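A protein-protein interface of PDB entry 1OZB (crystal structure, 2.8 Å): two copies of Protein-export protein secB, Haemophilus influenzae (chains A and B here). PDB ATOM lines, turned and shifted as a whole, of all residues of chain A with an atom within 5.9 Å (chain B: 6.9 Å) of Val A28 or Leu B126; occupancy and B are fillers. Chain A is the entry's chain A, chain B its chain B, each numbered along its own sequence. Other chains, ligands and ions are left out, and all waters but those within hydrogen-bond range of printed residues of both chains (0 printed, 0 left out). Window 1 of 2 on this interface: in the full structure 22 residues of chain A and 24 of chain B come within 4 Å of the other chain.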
ATOM      1  N   VAL A  25     -29.481   5.852 -10.037  1.00  0.00           N
ATOM      2  CA  VAL A  25     -29.082   7.222  -9.782  1.00  0.00           C
ATOM      3  C   VAL A  25     -30.204   8.132 -10.275  1.00  0.00           C
ATOM      4  O   VAL A  25     -30.682   7.964 -11.395  1.00  0.00           O
ATOM      5  CB  VAL A  25     -27.759   7.535 -10.556  1.00  0.00           C
ATOM      6  CG1 VAL A  25     -28.061   8.059 -11.944  1.00  0.00           C
ATOM      7  CG2 VAL A  25     -26.909   8.503  -9.789  1.00  0.00           C
ATOM      8  N   LYS A  26     -30.634   9.092  -9.463  1.00  0.00           N
ATOM      9  CA  LYS A  26     -31.708   9.993  -9.885  1.00  0.00           C
ATOM     10  C   LYS A  26     -31.157  11.289 -10.462  1.00  0.00           C
ATOM     11  O   LYS A  26     -31.753  11.889 -11.363  1.00  0.00           O
ATOM     12  CB  LYS A  26     -32.632  10.328  -8.716  1.00  0.00           C
ATOM     13  CG  LYS A  26     -33.250   9.106  -8.072  1.00  0.00           C
ATOM     14  CD  LYS A  26     -34.267   9.440  -6.998  1.00  0.00           C
ATOM     15  CE  LYS A  26     -35.570   9.914  -7.588  1.00  0.00           C
ATOM     16  NZ  LYS A  26     -36.620   9.886  -6.544  1.00  0.00           N
ATOM     17  N   ASP A  27     -30.013  11.720  -9.944  1.00  0.00           N
ATOM     18  CA  ASP A  27     -29.394  12.964 -10.394  1.00  0.00           C
ATOM     19  C   ASP A  27     -27.884  12.903 -10.186  1.00  0.00           C
ATOM     20  O   ASP A  27     -27.406  12.399  -9.160  1.00  0.00           O
ATOM     21  CB  ASP A  27     -29.988  14.149  -9.604  1.00  0.00           C
ATOM     22  CG  ASP A  27     -29.345  15.496  -9.959  1.00  0.00           C
ATOM     23  OD1 ASP A  27     -28.290  15.868  -9.379  1.00  0.00           O
ATOM     24  OD2 ASP A  27     -29.900  16.194 -10.828  1.00  0.00           O
ATOM     25  N   VAL A  28     -27.137  13.415 -11.160  1.00  0.00           N
ATOM     26  CA  VAL A  28     -25.687  13.434 -11.073  1.00  0.00           C
ATOM     27  C   VAL A  28     -25.164  14.746 -11.620  1.00  0.00           C
ATOM     28  O   VAL A  28     -25.667  15.248 -12.630  1.00  0.00           O
ATOM     29  CB  VAL A  28     -25.028  12.336 -11.922  1.00  0.00           C
ATOM     30  CG1 VAL A  28     -23.511  12.546 -11.903  1.00  0.00           C
ATOM     31  CG2 VAL A  28     -25.386  10.945 -11.393  1.00  0.00           C
ATOM     32  N   SER A  29     -24.139  15.293 -10.982  1.00  0.00           N
ATOM     33  CA  SER A  29     -23.563  16.532 -11.462  1.00  0.00           C
ATOM     34  C   SER A  29     -22.100  16.595 -11.071  1.00  0.00           C
ATOM     35  O   SER A  29     -21.742  16.295  -9.927  1.00  0.00           O
ATOM     36  CB  SER A  29     -24.315  17.716 -10.865  1.00  0.00           C
ATOM     37  OG  SER A  29     -23.912  18.938 -11.453  1.00  0.00           O
ATOM     38  N   PHE A  30     -21.250  16.956 -12.029  1.00  0.00           N
ATOM     39  CA  PHE A  30     -19.826  17.080 -11.764  1.00  0.00           C
ATOM     40  C   PHE A  30     -19.326  18.256 -12.569  1.00  0.00           C
ATOM     41  O   PHE A  30     -19.540  18.314 -13.792  1.00  0.00           O
ATOM     42  CB  PHE A  30     -19.058  15.837 -12.202  1.00  0.00           C
ATOM     43  CG  PHE A  30     -17.559  15.979 -12.078  1.00  0.00           C
ATOM     44  CD1 PHE A  30     -16.901  15.614 -10.905  1.00  0.00           C
ATOM     45  CD2 PHE A  30     -16.803  16.486 -13.131  1.00  0.00           C
ATOM     46  CE1 PHE A  30     -15.508  15.750 -10.791  1.00  0.00           C
ATOM     47  CE2 PHE A  30     -15.408  16.623 -13.017  1.00  0.00           C
ATOM     48  CZ  PHE A  30     -14.772  16.253 -11.847  1.00  0.00           C
ATOM     49  N   GLU A  86     -22.118  16.490  -7.120  1.00  0.00           N
ATOM     50  CA  GLU A  86     -23.370  16.235  -6.415  1.00  0.00           C
ATOM     51  C   GLU A  86     -24.011  14.962  -6.943  1.00  0.00           C
ATOM     52  O   GLU A  86     -24.177  14.782  -8.146  1.00  0.00           O
ATOM     53  CB  GLU A  86     -24.332  17.403  -6.601  1.00  0.00           C
ATOM     54  CG  GLU A  86     -24.376  18.346  -5.440  1.00  0.00           C
ATOM     55  CD  GLU A  86     -25.402  19.426  -5.644  1.00  0.00           C
ATOM     56  OE1 GLU A  86     -26.523  19.098  -6.093  1.00  0.00           O
ATOM     57  OE2 GLU A  86     -25.094  20.601  -5.349  1.00  0.00           O
ATOM     58  N   VAL A  87     -24.395  14.085  -6.039  1.00  0.00           N
ATOM     59  CA  VAL A  87     -24.973  12.840  -6.462  1.00  0.00           C
ATOM     60  C   VAL A  87     -26.198  12.483  -5.651  1.00  0.00           C
ATOM     61  O   VAL A  87     -26.245  12.719  -4.438  1.00  0.00           O
ATOM     62  CB  VAL A  87     -23.900  11.724  -6.374  1.00  0.00           C
ATOM     63  CG1 VAL A  87     -24.540  10.358  -6.368  1.00  0.00           C
ATOM     64  CG2 VAL A  87     -22.949  11.867  -7.565  1.00  0.00           C
ATOM     65  N   LYS A  88     -27.196  11.938  -6.342  1.00  0.00           N
ATOM     66  CA  LYS A  88     -28.420  11.499  -5.708  1.00  0.00           C
ATOM     67  C   LYS A  88     -28.519  10.007  -6.020  1.00  0.00           C
ATOM     68  O   LYS A  88     -29.029   9.614  -7.068  1.00  0.00           O
ATOM     69  CB  LYS A  88     -29.606  12.263  -6.281  1.00  0.00           C
ATOM     70  CG  LYS A  88     -30.545  12.794  -5.219  1.00  0.00           C
ATOM     71  CD  LYS A  88     -31.136  14.128  -5.638  1.00  0.00           C
ATOM     72  CE  LYS A  88     -32.011  14.712  -4.544  1.00  0.00           C
ATOM     73  NZ  LYS A  88     -32.350  16.137  -4.826  1.00  0.00           N
ATOM     74  N   LEU A 122     -19.370   6.116  -7.564  1.00  0.00           N
ATOM     75  CA  LEU A 122     -19.819   7.091  -8.552  1.00  0.00           C
ATOM     76  C   LEU A 122     -18.973   8.347  -8.435  1.00  0.00           C
ATOM     77  O   LEU A 122     -18.468   8.842  -9.444  1.00  0.00           O
ATOM     78  CB  LEU A 122     -21.297   7.427  -8.327  1.00  0.00           C
ATOM     79  CG  LEU A 122     -21.912   8.532  -9.193  1.00  0.00           C
ATOM     80  CD1 LEU A 122     -21.731   8.228 -10.674  1.00  0.00           C
ATOM     81  CD2 LEU A 122     -23.376   8.661  -8.850  1.00  0.00           C
ATOM     82  N   LEU A 126     -16.337   9.811 -11.325  1.00  0.00           N
ATOM     83  CA  LEU A 126     -16.418  11.159 -11.872  1.00  0.00           C
ATOM     84  C   LEU A 126     -15.160  11.977 -11.609  1.00  0.00           C
ATOM     85  O   LEU A 126     -14.671  12.654 -12.510  1.00  0.00           O
ATOM     86  CB  LEU A 126     -17.645  11.889 -11.304  1.00  0.00           C
ATOM     87  CG  LEU A 126     -19.006  11.354 -11.782  1.00  0.00           C
ATOM     88  CD1 LEU A 126     -20.108  11.811 -10.855  1.00  0.00           C
ATOM     89  CD2 LEU A 126     -19.253  11.791 -13.211  1.00  0.00           C
ATOM     90  N   VAL B  28     -20.587  17.644 -16.195  1.00  0.00           N
ATOM     91  CA  VAL B  28     -21.455  16.494 -16.446  1.00  0.00           C
ATOM     92  C   VAL B  28     -22.760  16.709 -15.718  1.00  0.00           C
ATOM     93  O   VAL B  28     -22.776  17.226 -14.598  1.00  0.00           O
ATOM     94  CB  VAL B  28     -20.923  15.163 -15.862  1.00  0.00           C
ATOM     95  CG1 VAL B  28     -21.694  14.003 -16.442  1.00  0.00           C
ATOM     96  CG2 VAL B  28     -19.474  15.017 -16.108  1.00  0.00           C
ATOM     97  N   SER B  29     -23.842  16.263 -16.343  1.00  0.00           N
ATOM     98  CA  SER B  29     -25.176  16.359 -15.770  1.00  0.00           C
ATOM     99  C   SER B  29     -25.988  15.179 -16.245  1.00  0.00           C
ATOM    100  O   SER B  29     -25.965  14.847 -17.434  1.00  0.00           O
ATOM    101  CB  SER B  29     -25.901  17.620 -16.237  1.00  0.00           C
ATOM    102  OG  SER B  29     -25.460  18.767 -15.553  1.00  0.00           O
ATOM    103  N   PHE B  30     -26.699  14.544 -15.323  1.00  0.00           N
ATOM    104  CA  PHE B  30     -27.572  13.441 -15.683  1.00  0.00           C
ATOM    105  C   PHE B  30     -28.748  13.524 -14.748  1.00  0.00           C
ATOM    106  O   PHE B  30     -28.569  13.532 -13.527  1.00  0.00           O
ATOM    107  CB  PHE B  30     -26.892  12.076 -15.529  1.00  0.00           C
ATOM    108  CG  PHE B  30     -27.822  10.912 -15.785  1.00  0.00           C
ATOM    109  CD1 PHE B  30     -28.079  10.478 -17.076  1.00  0.00           C
ATOM    110  CD2 PHE B  30     -28.451  10.264 -14.732  1.00  0.00           C
ATOM    111  CE1 PHE B  30     -28.954   9.408 -17.308  1.00  0.00           C
ATOM    112  CE2 PHE B  30     -29.327   9.192 -14.968  1.00  0.00           C
ATOM    113  CZ  PHE B  30     -29.571   8.770 -16.253  1.00  0.00           C
ATOM    114  N   GLU B  31     -29.945  13.583 -15.322  1.00  0.00           N
ATOM    115  CA  GLU B  31     -31.156  13.696 -14.531  1.00  0.00           C
ATOM    116  C   GLU B  31     -32.217  12.702 -14.949  1.00  0.00           C
ATOM    117  O   GLU B  31     -32.477  12.523 -16.137  1.00  0.00           O
ATOM    118  CB  GLU B  31     -31.715  15.106 -14.658  1.00  0.00           C
ATOM    119  CG  GLU B  31     -30.653  16.183 -14.597  1.00  0.00           C
ATOM    120  CD  GLU B  31     -31.243  17.578 -14.556  1.00  0.00           C
ATOM    121  OE1 GLU B  31     -31.867  17.928 -13.528  1.00  0.00           O
ATOM    122  OE2 GLU B  31     -31.086  18.319 -15.552  1.00  0.00           O
ATOM    123  N   ALA B  32     -32.824  12.063 -13.952  1.00  0.00           N
ATOM    124  CA  ALA B  32     -33.880  11.088 -14.159  1.00  0.00           C
ATOM    125  C   ALA B  32     -35.015  11.502 -13.224  1.00  0.00           C
ATOM    126  O   ALA B  32     -35.224  10.897 -12.167  1.00  0.00           O
ATOM    127  CB  ALA B  32     -33.381   9.705 -13.811  1.00  0.00           C
ATOM    128  N   CYS B  85     -29.146  13.962 -20.273  1.00  0.00           N
ATOM    129  CA  CYS B  85     -27.733  13.838 -19.984  1.00  0.00           C
ATOM    130  C   CYS B  85     -26.923  14.816 -20.824  1.00  0.00           C
ATOM    131  O   CYS B  85     -27.013  14.809 -22.051  1.00  0.00           O
ATOM    132  CB  CYS B  85     -27.261  12.412 -20.254  1.00  0.00           C
ATOM    133  SG  CYS B  85     -25.523  12.140 -19.858  1.00  0.00           S
ATOM    134  N   GLU B  86     -26.144  15.666 -20.157  1.00  0.00           N
ATOM    135  CA  GLU B  86     -25.304  16.639 -20.839  1.00  0.00           C
ATOM    136  C   GLU B  86     -23.876  16.417 -20.402  1.00  0.00           C
ATOM    137  O   GLU B  86     -23.596  16.307 -19.212  1.00  0.00           O
ATOM    138  CB  GLU B  86     -25.721  18.061 -20.495  1.00  0.00           C
ATOM    139  CG  GLU B  86     -27.150  18.370 -20.840  1.00  0.00           C
ATOM    140  CD  GLU B  86     -27.486  19.827 -20.626  1.00  0.00           C
ATOM    141  OE1 GLU B  86     -27.280  20.327 -19.496  1.00  0.00           O
ATOM    142  OE2 GLU B  86     -27.957  20.470 -21.591  1.00  0.00           O
ATOM    143  N   VAL B  87     -22.978  16.344 -21.376  1.00  0.00           N
ATOM    144  CA  VAL B  87     -21.560  16.129 -21.121  1.00  0.00           C
ATOM    145  C   VAL B  87     -20.688  17.146 -21.851  1.00  0.00           C
ATOM    146  O   VAL B  87     -20.927  17.464 -23.024  1.00  0.00           O
ATOM    147  CB  VAL B  87     -21.125  14.724 -21.575  1.00  0.00           C
ATOM    148  CG1 VAL B  87     -19.602  14.653 -21.684  1.00  0.00           C
ATOM    149  CG2 VAL B  87     -21.616  13.684 -20.582  1.00  0.00           C
ATOM    150  N   GLU B 121     -18.731   6.924 -23.835  1.00  0.00           N
ATOM    151  CA  GLU B 121     -18.612   6.042 -22.682  1.00  0.00           C
ATOM    152  C   GLU B 121     -19.175   6.701 -21.427  1.00  0.00           C
ATOM    153  O   GLU B 121     -19.739   6.017 -20.576  1.00  0.00           O
ATOM    154  CB  GLU B 121     -17.134   5.643 -22.473  1.00  0.00           C
ATOM    155  CG  GLU B 121     -16.911   4.522 -21.454  1.00  0.00           C
ATOM    156  CD  GLU B 121     -17.046   4.992 -20.018  1.00  0.00           C
ATOM    157  OE1 GLU B 121     -17.446   4.178 -19.142  1.00  0.00           O
ATOM    158  OE2 GLU B 121     -16.738   6.185 -19.770  1.00  0.00           O
ATOM    159  N   LEU B 122     -19.026   8.024 -21.308  1.00  0.00           N
ATOM    160  CA  LEU B 122     -19.544   8.726 -20.133  1.00  0.00           C
ATOM    161  C   LEU B 122     -21.052   8.726 -20.171  1.00  0.00           C
ATOM    162  O   LEU B 122     -21.702   8.519 -19.149  1.00  0.00           O
ATOM    163  CB  LEU B 122     -19.038  10.176 -20.044  1.00  0.00           C
ATOM    164  CG  LEU B 122     -19.665  10.976 -18.878  1.00  0.00           C
ATOM    165  CD1 LEU B 122     -19.500  10.220 -17.559  1.00  0.00           C
ATOM    166  CD2 LEU B 122     -19.044  12.351 -18.790  1.00  0.00           C
ATOM    167  N   VAL B 123     -21.615   8.960 -21.349  1.00  0.00           N
ATOM    168  CA  VAL B 123     -23.063   8.937 -21.479  1.00  0.00           C
ATOM    169  C   VAL B 123     -23.586   7.531 -21.171  1.00  0.00           C
ATOM    170  O   VAL B 123     -24.529   7.381 -20.398  1.00  0.00           O
ATOM    171  CB  VAL B 123     -23.535   9.309 -22.890  1.00  0.00           C
ATOM    172  CG1 VAL B 123     -25.069   9.217 -22.954  1.00  0.00           C
ATOM    173  CG2 VAL B 123     -23.051  10.709 -23.257  1.00  0.00           C
ATOM    174  N   SER B 124     -22.979   6.502 -21.757  1.00  0.00           N
ATOM    175  CA  SER B 124     -23.440   5.146 -21.496  1.00  0.00           C
ATOM    176  C   SER B 124     -23.308   4.774 -20.012  1.00  0.00           C
ATOM    177  O   SER B 124     -24.177   4.110 -19.433  1.00  0.00           O
ATOM    178  CB  SER B 124     -22.689   4.128 -22.367  1.00  0.00           C
ATOM    179  OG  SER B 124     -21.327   4.046 -22.012  1.00  0.00           O
ATOM    180  N   ASN B 125     -22.230   5.213 -19.389  1.00  0.00           N
ATOM    181  CA  ASN B 125     -21.980   4.907 -17.996  1.00  0.00           C
ATOM    182  C   ASN B 125     -23.111   5.465 -17.130  1.00  0.00           C
ATOM    183  O   ASN B 125     -23.718   4.740 -16.330  1.00  0.00           O
ATOM    184  CB  ASN B 125     -20.640   5.518 -17.610  1.00  0.00           C
ATOM    185  CG  ASN B 125     -20.064   4.909 -16.385  1.00  0.00           C
ATOM    186  OD1 ASN B 125     -20.652   4.987 -15.313  1.00  0.00           O
ATOM    187  ND2 ASN B 125     -18.886   4.285 -16.524  1.00  0.00           N
ATOM    188  N   LEU B 126     -23.405   6.754 -17.314  1.00  0.00           N
ATOM    189  CA  LEU B 126     -24.457   7.424 -16.555  1.00  0.00           C
ATOM    190  C   LEU B 126     -25.848   6.840 -16.794  1.00  0.00           C
ATOM    191  O   LEU B 126     -26.619   6.656 -15.851  1.00  0.00           O
ATOM    192  CB  LEU B 126     -24.476   8.916 -16.883  1.00  0.00           C
ATOM    193  CG  LEU B 126     -23.297   9.712 -16.318  1.00  0.00           C
ATOM    194  CD1 LEU B 126     -23.132  11.031 -17.064  1.00  0.00           C
ATOM    195  CD2 LEU B 126     -23.519   9.931 -14.827  1.00  0.00           C
ATOM    196  N   VAL B 127     -26.181   6.552 -18.049  1.00  0.00           N
ATOM    197  CA  VAL B 127     -27.497   5.993 -18.334  1.00  0.00           C
ATOM    198  C   VAL B 127     -27.655   4.651 -17.635  1.00  0.00           C
ATOM    199  O   VAL B 127     -28.684   4.389 -17.017  1.00  0.00           O
ATOM    200  CB  VAL B 127     -27.741   5.848 -19.846  1.00  0.00           C
ATOM    201  CG1 VAL B 127     -29.076   5.169 -20.104  1.00  0.00           C
ATOM    202  CG2 VAL B 127     -27.754   7.226 -20.492  1.00  0.00           C
ATOM    203  N   ASN B 128     -26.627   3.808 -17.708  1.00  0.00           N
ATOM    204  CA  ASN B 128     -26.669   2.507 -17.052  1.00  0.00           C
ATOM    205  C   ASN B 128     -26.886   2.687 -15.541  1.00  0.00           C
ATOM    206  O   ASN B 128     -27.540   1.866 -14.919  1.00  0.00           O
ATOM    207  CB  ASN B 128     -25.369   1.741 -17.338  1.00  0.00           C
ATOM    208  CG  ASN B 128     -25.326   0.362 -16.671  1.00  0.00           C
ATOM    209  OD1 ASN B 128     -26.144  -0.516 -16.961  1.00  0.00           O
ATOM    210  ND2 ASN B 128     -24.357   0.169 -15.781  1.00  0.00           N
ATOM    211  N   ARG B 129     -26.353   3.758 -14.957  1.00  0.00           N
ATOM    212  CA  ARG B 129     -26.523   3.985 -13.530  1.00  0.00           C
ATOM    213  C   ARG B 129     -27.965   4.326 -13.179  1.00  0.00           C
ATOM    214  O   ARG B 129     -28.373   4.200 -12.024  1.00  0.00           O
ATOM    215  CB  ARG B 129     -25.579   5.074 -13.066  1.00  0.00           C
ATOM    216  CG  ARG B 129     -24.128   4.633 -13.065  1.00  0.00           C
ATOM    217  CD  ARG B 129     -23.206   5.799 -12.767  1.00  0.00           C
ATOM    218  NE  ARG B 129     -21.812   5.413 -12.861  1.00  0.00           N
ATOM    219  CZ  ARG B 129     -21.124   4.861 -11.872  1.00  0.00           C
ATOM    220  NH1 ARG B 129     -21.721   4.641 -10.712  1.00  0.00           N
ATOM    221  NH2 ARG B 129     -19.839   4.526 -12.052  1.00  0.00           N
ATOM    222  N   GLY B 130     -28.739   4.751 -14.172  1.00  0.00           N
ATOM    223  CA  GLY B 130     -30.138   5.043 -13.917  1.00  0.00           C
ATOM    224  C   GLY B 130     -30.960   3.805 -14.241  1.00  0.00           C
ATOM    225  O   GLY B 130     -32.182   3.841 -14.229  1.00  0.00           O
ATOM    226  N   THR B 131     -30.258   2.701 -14.510  1.00  0.00           N
ATOM    227  CA  THR B 131     -30.828   1.405 -14.880  1.00  0.00           C
ATOM    228  C   THR B 131     -31.740   1.488 -16.088  1.00  0.00           C
ATOM    229  O   THR B 131     -32.793   0.869 -16.135  1.00  0.00           O
ATOM    230  CB  THR B 131     -31.593   0.696 -13.713  1.00  0.00           C
ATOM    231  OG1 THR B 131     -32.729   1.468 -13.300  1.00  0.00           O
ATOM    232  CG2 THR B 131     -30.662   0.467 -12.541  1.00  0.00           C
ATOM    233  N   PHE B 132     -31.330   2.263 -17.073  1.00  0.00           N
ATOM    234  CA  PHE B 132     -32.113   2.375 -18.286  1.00  0.00           C
ATOM    235  C   PHE B 132     -31.428   1.461 -19.281  1.00  0.00           C
ATOM    236  O   PHE B 132     -30.248   1.153 -19.140  1.00  0.00           O
ATOM    237  CB  PHE B 132     -32.098   3.819 -18.822  1.00  0.00           C
ATOM    238  CG  PHE B 132     -32.875   4.777 -17.990  1.00  0.00           C
ATOM    239  CD1 PHE B 132     -32.233   5.741 -17.246  1.00  0.00           C
ATOM    240  CD2 PHE B 132     -34.260   4.673 -17.908  1.00  0.00           C
ATOM    241  CE1 PHE B 132     -32.952   6.589 -16.424  1.00  0.00           C
ATOM    242  CE2 PHE B 132     -34.994   5.516 -17.087  1.00  0.00           C
ATOM    243  CZ  PHE B 132     -34.341   6.475 -16.341  1.00  0.00           C
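The backbone NH (N) of Ala B32 sits at hydrogen-bond distance from the backbone carbonyl oxygen (O) of Lys A26 (2.8 Å).
The backbone NH (N) of Val A25 lies within hydrogen-bond range of the backbone carbonyl oxygen (O) of Arg B129 (2.8 Å).
The backbone NH (N) of Val A28 sits at hydrogen-bond distance from the backbone carbonyl oxygen (O) of Phe B30 (2.8 Å).
The backbone NH of Val B28 lies within hydrogen-bond range of the backbone carbonyl oxygen of Phe A30, 2.7 Å away.
OD1 of Asn B125 lies within hydrogen-bond range of NE of Arg B129 (2.7 Å).
The backbone carbonyl oxygen of Ser A29 lies within hydrogen-bond range of the backbone NH of Glu A86, at 2.8 Å.
The backbone carbonyl oxygen of Ser B29 lies within hydrogen-bond range of the backbone NH of Glu B86, 2.8 Å away.
The side-chain sulfur of Cys B85 lies close to the backbone carbonyl oxygen of Ser B29, at 3.7 Å.
N of Lys A26 sits at hydrogen-bond distance from O of Lys A88 (2.9 Å).
The backbone carbonyl oxygen (O) of Asp A27 is in hydrogen-bond range of the backbone NH (N) of Lys A88.
Phe B30 touches Val A25.
CA of Gly B130 touches O of Val A25, at 3.9 Å.
Lys A26 touches Glu B31 (O to CA, 3.7 Å).
O of Phe B30 touches CA of Asp A27, 3.3 Å away.
Asp A27 touches Glu B31.
Val A28 touches Ser B29 (O to CA, 3.4 Å).
Val A28 touches Leu B126 (CG1 to CD2, 3.9 Å).
O of Val B28 touches CA of Ser A29, 3.3 Å away.
Leu A122 touches Arg B129 (CD1 to CD, 3.5 Å).
Of the printed residues of chain B, Val A25 touches Phe B30, Arg B129 and Gly B130.
Of the printed residues of chain B, Val A28 touches Ser B29 (3.4 Å), Phe B30 (2.8 Å) and Leu B126 (3.9 Å).
Of the printed residues of chain A, Val B28 touches Ser A29 and Phe A30.
Of the printed residues of chain A, Phe B30 touches Val A25, Asp A27 and Val A28.
Of the printed residues of chain A, Glu B31 touches Lys A26 (3.7 Å) and Asp A27 (3.8 Å).
Of chain A, only Val A28 (3.9 Å) comes within 4 Å of Leu B126.
Asn B128 touches none of the printed residues of chain A.
Of the printed residues of chain A, Arg B129 touches Val A25 and Leu A122.
The nearest printed residue of chain B that does not touch Val A28 is Val B28 (4.02 Å).
Of the 20 printed residues of chain B, 8 touch a printed residue of chain A.
Of the 11 printed residues of chain A, 7 touch a printed residue of chain B.
Hydrophobic or aromatic side chains of chain A that line the printed part of chain B: Val A25, Val A28 and Leu A122.
Among the printed residues, 13 pairs touch across the chains.
Val A28 touches Ser B29, and with the chains exchanged Ser A29 touches Val B28.
Val A28 touches Phe B30, and with the chains exchanged Phe A30 touches Val B28.
Val A28 touches Leu B126, but with the chains exchanged Leu A126 does not touch Val B28 (4.3 Å).
Of the 13 pairs that touch across the chains among the printed residues, 4 have their exchanged pair printed and touching as well.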
